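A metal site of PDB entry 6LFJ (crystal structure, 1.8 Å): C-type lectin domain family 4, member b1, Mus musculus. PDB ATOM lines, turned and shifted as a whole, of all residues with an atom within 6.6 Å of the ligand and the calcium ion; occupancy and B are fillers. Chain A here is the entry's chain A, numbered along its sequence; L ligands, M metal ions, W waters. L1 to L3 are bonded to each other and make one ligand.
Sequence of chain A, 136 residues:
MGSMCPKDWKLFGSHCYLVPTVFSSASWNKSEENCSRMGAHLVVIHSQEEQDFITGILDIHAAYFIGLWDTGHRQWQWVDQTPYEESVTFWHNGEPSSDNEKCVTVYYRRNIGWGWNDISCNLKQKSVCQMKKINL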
ATOM      1  N   GLY A  94     -36.204   4.887  26.312  1.00  0.00           N
ATOM      2  CA  GLY A  94     -36.011   4.351  27.672  1.00  0.00           C
ATOM      3  C   GLY A  94     -34.555   4.278  28.084  1.00  0.00           C
ATOM      4  O   GLY A  94     -34.260   3.749  29.160  1.00  0.00           O
ATOM      5  N   GLU A  95     -33.629   4.774  27.245  1.00  0.00           N
ATOM      6  CA  GLU A  95     -32.193   4.838  27.573  1.00  0.00           C
ATOM      7  C   GLU A  95     -31.769   6.300  27.662  1.00  0.00           C
ATOM      8  O   GLU A  95     -32.353   7.164  27.015  1.00  0.00           O
ATOM      9  CB  GLU A  95     -31.338   4.085  26.553  1.00  0.00           C
ATOM     10  CG  GLU A  95     -31.774   2.650  26.335  1.00  0.00           C
ATOM     11  CD  GLU A  95     -31.732   1.726  27.548  1.00  0.00           C
ATOM     12  OE1 GLU A  95     -31.019   2.030  28.504  1.00  0.00           O
ATOM     13  OE2 GLU A  95     -32.398   0.670  27.500  1.00  0.00           O
ATOM     14  N   PRO A  96     -30.761   6.658  28.494  1.00  0.00           N
ATOM     15  CA  PRO A  96     -30.151   5.737  29.449  1.00  0.00           C
ATOM     16  C   PRO A  96     -31.107   5.298  30.553  1.00  0.00           C
ATOM     17  O   PRO A  96     -32.048   5.993  30.835  1.00  0.00           O
ATOM     18  CB  PRO A  96     -29.060   6.571  30.128  1.00  0.00           C
ATOM     19  CG  PRO A  96     -28.832   7.745  29.226  1.00  0.00           C
ATOM     20  CD  PRO A  96     -30.142   7.984  28.515  1.00  0.00           C
ATOM     21  N   SER A  97     -30.812   4.164  31.197  1.00  0.00           N
ATOM     22  CA  SER A  97     -31.769   3.458  32.074  1.00  0.00           C
ATOM     23  C   SER A  97     -31.267   3.376  33.509  1.00  0.00           C
ATOM     24  O   SER A  97     -32.121   3.144  34.355  1.00  0.00           O
ATOM     25  CB  SER A  97     -32.058   2.083  31.540  1.00  0.00           C
ATOM     26  OG  SER A  97     -30.902   1.244  31.638  1.00  0.00           O
ATOM     27  N   SER A  98     -29.977   3.499  33.798  1.00  0.00           N
ATOM     28  CA  SER A  98     -29.437   3.129  35.134  1.00  0.00           C
ATOM     29  C   SER A  98     -28.119   3.823  35.481  1.00  0.00           C
ATOM     30  O   SER A  98     -27.133   3.677  34.728  1.00  0.00           O
ATOM     31  CB  SER A  98     -29.295   1.629  35.202  1.00  0.00           C
ATOM     32  OG  SER A  98     -28.568   1.263  36.360  1.00  0.00           O
ATOM     33  N   ASN A 100     -26.035   2.787  37.409  1.00  0.00           N
ATOM     34  CA  ASN A 100     -25.031   1.708  37.600  1.00  0.00           C
ATOM     35  C   ASN A 100     -24.417   1.292  36.250  1.00  0.00           C
ATOM     36  O   ASN A 100     -23.439   0.553  36.284  1.00  0.00           O
ATOM     37  CB  ASN A 100     -25.622   0.499  38.323  1.00  0.00           C
ATOM     38  CG  ASN A 100     -24.579  -0.208  39.169  1.00  0.00           C
ATOM     39  OD1 ASN A 100     -23.632   0.421  39.647  1.00  0.00           O
ATOM     40  ND2 ASN A 100     -24.754  -1.500  39.360  1.00  0.00           N
ATOM     41  N   GLU A 101     -24.975   1.753  35.127  1.00  0.00           N
ATOM     42  CA  GLU A 101     -24.499   1.431  33.764  1.00  0.00           C
ATOM     43  C   GLU A 101     -23.694   2.625  33.225  1.00  0.00           C
ATOM     44  O   GLU A 101     -24.316   3.644  32.831  1.00  0.00           O
ATOM     45  CB  GLU A 101     -25.690   1.066  32.863  1.00  0.00           C
ATOM     46  CG  GLU A 101     -26.348  -0.265  33.229  1.00  0.00           C
ATOM     47  CD  GLU A 101     -27.539  -0.655  32.372  1.00  0.00           C
ATOM     48  OE1 GLU A 101     -28.325   0.257  31.983  1.00  0.00           O
ATOM     49  OE2 GLU A 101     -27.695  -1.870  32.058  1.00  0.00           O
ATOM     50  N   TYR A 107     -26.691  -0.725  19.376  1.00  0.00           N
ATOM     51  CA  TYR A 107     -27.284  -1.997  18.882  1.00  0.00           C
ATOM     52  C   TYR A 107     -28.609  -1.691  18.174  1.00  0.00           C
ATOM     53  O   TYR A 107     -29.163  -0.582  18.292  1.00  0.00           O
ATOM     54  CB  TYR A 107     -27.415  -3.008  20.027  1.00  0.00           C
ATOM     55  CG  TYR A 107     -28.677  -2.879  20.839  1.00  0.00           C
ATOM     56  CD1 TYR A 107     -28.782  -1.923  21.827  1.00  0.00           C
ATOM     57  CD2 TYR A 107     -29.758  -3.703  20.597  1.00  0.00           C
ATOM     58  CE1 TYR A 107     -29.937  -1.796  22.588  1.00  0.00           C
ATOM     59  CE2 TYR A 107     -30.927  -3.585  21.342  1.00  0.00           C
ATOM     60  CZ  TYR A 107     -31.016  -2.632  22.338  1.00  0.00           C
ATOM     61  OH  TYR A 107     -32.146  -2.493  23.090  1.00  0.00           O
ATOM     62  N   ARG A 109     -32.522  -2.413  17.364  1.00  0.00           N
ATOM     63  CA  ARG A 109     -33.836  -2.934  17.822  1.00  0.00           C
ATOM     64  C   ARG A 109     -34.690  -3.249  16.594  1.00  0.00           C
ATOM     65  O   ARG A 109     -34.821  -2.375  15.719  1.00  0.00           O
ATOM     66  CB  ARG A 109     -34.519  -1.906  18.733  1.00  0.00           C
ATOM     67  CG  ARG A 109     -33.940  -1.821  20.138  1.00  0.00           C
ATOM     68  CD  ARG A 109     -34.834  -1.012  21.068  1.00  0.00           C
ATOM     69  NE  ARG A 109     -34.304  -0.881  22.416  1.00  0.00           N
ATOM     70  CZ  ARG A 109     -34.810  -0.088  23.354  1.00  0.00           C
ATOM     71  NH1 ARG A 109     -35.853   0.671  23.107  1.00  0.00           N
ATOM     72  NH2 ARG A 109     -34.259  -0.046  24.554  1.00  0.00           N
ATOM     73  N   ASN A 117     -27.412   2.374  24.180  1.00  0.00           N
ATOM     74  CA  ASN A 117     -27.860   1.772  25.448  1.00  0.00           C
ATOM     75  C   ASN A 117     -26.721   1.900  26.461  1.00  0.00           C
ATOM     76  O   ASN A 117     -25.587   1.504  26.149  1.00  0.00           O
ATOM     77  CB  ASN A 117     -28.252   0.304  25.247  1.00  0.00           C
ATOM     78  CG  ASN A 117     -28.651  -0.348  26.555  1.00  0.00           C
ATOM     79  OD1 ASN A 117     -29.218   0.311  27.417  1.00  0.00           O
ATOM     80  ND2 ASN A 117     -28.364  -1.642  26.697  1.00  0.00           N
ATOM     81  N   ASP A 118     -27.015   2.414  27.651  1.00  0.00           N
ATOM     82  CA  ASP A 118     -26.034   2.360  28.763  1.00  0.00           C
ATOM     83  C   ASP A 118     -25.994   0.916  29.276  1.00  0.00           C
ATOM     84  O   ASP A 118     -27.065   0.282  29.406  1.00  0.00           O
ATOM     85  CB  ASP A 118     -26.333   3.393  29.851  1.00  0.00           C
ATOM     86  CG  ASP A 118     -27.679   3.286  30.527  1.00  0.00           C
ATOM     87  OD1 ASP A 118     -28.611   2.727  29.907  1.00  0.00           O
ATOM     88  OD2 ASP A 118     -27.803   3.804  31.659  1.00  0.00           O
ATOM     89  N   ILE A 119     -24.790   0.412  29.516  1.00  0.00           N
ATOM     90  CA  ILE A 119     -24.581  -0.982  30.019  1.00  0.00           C
ATOM     91  C   ILE A 119     -23.380  -1.014  30.949  1.00  0.00           C
ATOM     92  O   ILE A 119     -22.624  -0.038  31.005  1.00  0.00           O
ATOM     93  CB  ILE A 119     -24.398  -2.021  28.888  1.00  0.00           C
ATOM     94  CG1 ILE A 119     -23.153  -1.755  28.035  1.00  0.00           C
ATOM     95  CG2 ILE A 119     -25.645  -2.158  28.044  1.00  0.00           C
ATOM     96  CD1 ILE A 119     -22.616  -3.019  27.396  1.00  0.00           C
ATOM     97  N   SER A 120     -23.277  -2.112  31.685  1.00  0.00           N
ATOM     98  CA  SER A 120     -22.124  -2.394  32.575  1.00  0.00           C
ATOM     99  C   SER A 120     -20.845  -2.406  31.734  1.00  0.00           C
ATOM    100  O   SER A 120     -20.799  -3.137  30.713  1.00  0.00           O
ATOM    101  CB  SER A 120     -22.317  -3.688  33.315  1.00  0.00           C
ATOM    102  OG  SER A 120     -21.071  -4.177  33.787  1.00  0.00           O
ATOM    103  N   LEU A 123     -19.303  -5.987  30.983  1.00  0.00           N
ATOM    104  CA  LEU A 123     -19.875  -6.933  29.994  1.00  0.00           C
ATOM    105  C   LEU A 123     -19.015  -6.939  28.737  1.00  0.00           C
ATOM    106  O   LEU A 123     -18.529  -5.876  28.345  1.00  0.00           O
ATOM    107  CB  LEU A 123     -21.308  -6.522  29.656  1.00  0.00           C
ATOM    108  CG  LEU A 123     -22.334  -6.746  30.760  1.00  0.00           C
ATOM    109  CD1 LEU A 123     -23.713  -6.316  30.285  1.00  0.00           C
ATOM    110  CD2 LEU A 123     -22.352  -8.196  31.244  1.00  0.00           C
HETATM  111  C1  LIG L   1     -28.479  -6.986  33.451  1.00  0.00           C
HETATM  112  C2  LIG L   1     -27.684  -8.259  33.857  1.00  0.00           C
HETATM  113  C3  LIG L   1     -27.405  -8.214  35.346  1.00  0.00           C
HETATM  114  C4  LIG L   1     -26.608  -6.942  35.670  1.00  0.00           C
HETATM  115  C5  LIG L   1     -27.442  -5.725  35.242  1.00  0.00           C
HETATM  116  C6  LIG L   1     -26.692  -4.398  35.464  1.00  0.00           C
HETATM  117  O1  LIG L   1     -26.428  -8.346  33.129  1.00  0.00           O
HETATM  118  O2  LIG L   1     -26.649  -9.381  35.726  1.00  0.00           O
HETATM  119  O3  LIG L   1     -26.371  -6.919  37.062  1.00  0.00           O
HETATM  120  O4  LIG L   1     -27.752  -5.785  33.824  1.00  0.00           O
HETATM  121  O5  LIG L   1     -25.641  -4.263  34.477  1.00  0.00           O
HETATM  122  C1  LG2 L   2     -31.437  -6.917  32.160  1.00  0.00           C
HETATM  123  C2  LG2 L   2     -32.405  -6.013  31.384  1.00  0.00           C
HETATM  124  C3  LG2 L   2     -33.500  -5.539  32.319  1.00  0.00           C
HETATM  125  C4  LG2 L   2     -32.857  -4.807  33.501  1.00  0.00           C
HETATM  126  C5  LG2 L   2     -31.891  -5.704  34.270  1.00  0.00           C
HETATM  127  C6  LG2 L   2     -30.798  -6.167  33.343  1.00  0.00           C
HETATM  128  P1  LG2 L   2     -30.450  -8.690  30.594  1.00  0.00           P
HETATM  129  O1  LG2 L   2     -30.396  -7.299  31.293  1.00  0.00           O
HETATM  130  O2  LG2 L   2     -31.700  -4.845  30.910  1.00  0.00           O
HETATM  131  O3  LG2 L   2     -34.389  -4.651  31.603  1.00  0.00           O
HETATM  132  O4  LG2 L   2     -33.870  -4.353  34.378  1.00  0.00           O
HETATM  133  O5  LG2 L   2     -31.307  -4.930  35.317  1.00  0.00           O
HETATM  134  O6  LG2 L   2     -29.844  -7.028  34.040  1.00  0.00           O
HETATM  135  O7  LG2 L   2     -31.876  -8.697  29.785  1.00  0.00           O
HETATM  136  O8  LG2 L   2     -30.265  -9.818  31.558  1.00  0.00           O
HETATM  137  O9  LG2 L   2     -29.251  -8.524  29.511  1.00  0.00           O
HETATM  138  C1  LG3 L   3     -31.083  -4.903  29.628  1.00  0.00           C
HETATM  139  C2  LG3 L   3     -29.794  -4.045  29.660  1.00  0.00           C
HETATM  140  C3  LG3 L   3     -30.152  -2.577  29.958  1.00  0.00           C
HETATM  141  C4  LG3 L   3     -31.167  -2.083  28.995  1.00  0.00           C
HETATM  142  C5  LG3 L   3     -32.393  -2.993  28.987  1.00  0.00           C
HETATM  143  C6  LG3 L   3     -33.266  -2.667  27.765  1.00  0.00           C
HETATM  144  O1  LG3 L   3     -29.110  -4.133  28.430  1.00  0.00           O
HETATM  145  O2  LG3 L   3     -28.992  -1.813  29.870  1.00  0.00           O
HETATM  146  O3  LG3 L   3     -31.589  -0.794  29.400  1.00  0.00           O
HETATM  147  O4  LG3 L   3     -32.044  -4.347  28.727  1.00  0.00           O
HETATM  148  O5  LG3 L   3     -34.548  -3.256  27.948  1.00  0.00           O
HETATM  149 CA    CA M   1     -29.434   0.614  29.817  1.00  0.00          CA
HETATM  150  O   HOH W   1     -31.966  -0.735  25.237  1.00  0.00           O
HETATM  151  O   HOH W   2     -28.202  -1.576  36.396  1.00  0.00           O
HETATM  152  O   HOH W   3     -33.696  -1.150  31.653  1.00  0.00           O
HETATM  153  O   HOH W   4     -29.592  -2.496  33.908  1.00  0.00           O
HETATM  154  O   HOH W   5     -25.719  -3.666  32.083  1.00  0.00           O
HETATM  155  O   HOH W   6     -30.610  -4.118  25.719  1.00  0.00           O
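Water W5 lies within hydrogen-bond range of an oxygen (O5) of LIG L1 (2.5 Å), the side-chain carboxylate of Glu 101 (2.7 Å) and the backbone NH of Ser 120 (2.9 Å).
Water W6 lies within hydrogen-bond range of an oxygen (O1) of LG3 L3 (3.1 Å), the side-chain hydroxyl (OH) of Tyr 107 (3.5 Å) and the side-chain amide nitrogen (ND2) of Asn 117 (3.5 Å).
Water W4 lies within hydrogen-bond range of the side-chain carboxylate (OE2) of Glu 101 and an oxygen (O5) of LG2 L2.
Water W1 lies within hydrogen-bond range of NH2 of Arg 109, OE2 of Glu 95 and OH of Tyr 107.
OD2 of Asp 118 sits at hydrogen-bond distance from N of Ser 98 (3.1 Å).
The side-chain carboxylate (OE2) of Glu 95 lies within salt-bridge range of the guanidinium group (NH2) of Arg 109 (3.6 Å).
Within 4 Å of the calcium ion: Glu 95, Ser 97, Glu 101, Asn 117 and Asp 118.
The nearest printed residue that does not touch the calcium ion is Ile 119 (4.7 Å).
Residues that only touch the ligand: Ser 120 and Ile 119.
Within 4 Å of the ligand: Glu 95, Ser 97, Glu 101, Asn 117, Asp 118, Ile 119 and Ser 120.
Along chain A the residues within 4 Å of the ligand span positions 95 to 120.
The side-chain carboxylate (OD1) of Asp 118 is bound to the calcium ion, 2.3 Å away.
OG of Ser 97 is bound to the calcium ion.
The calcium ion is bound by O of Asp 118, 2.4 Å away.
The side-chain amide oxygen (OD1) of Asn 117 binds the calcium ion, at 2.4 Å.
The calcium ion is bound by the side-chain carboxylate (OE1) of Glu 101, 2.5 Å away.
The calcium ion is bound by O2 of LG3 L3, 2.5 Å away.
The calcium ion is bound by the side-chain carboxylate (OE1) of Glu 95 (2.5 Å).
O3 of LG3 L3 is bound to the calcium ion (2.6 Å).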
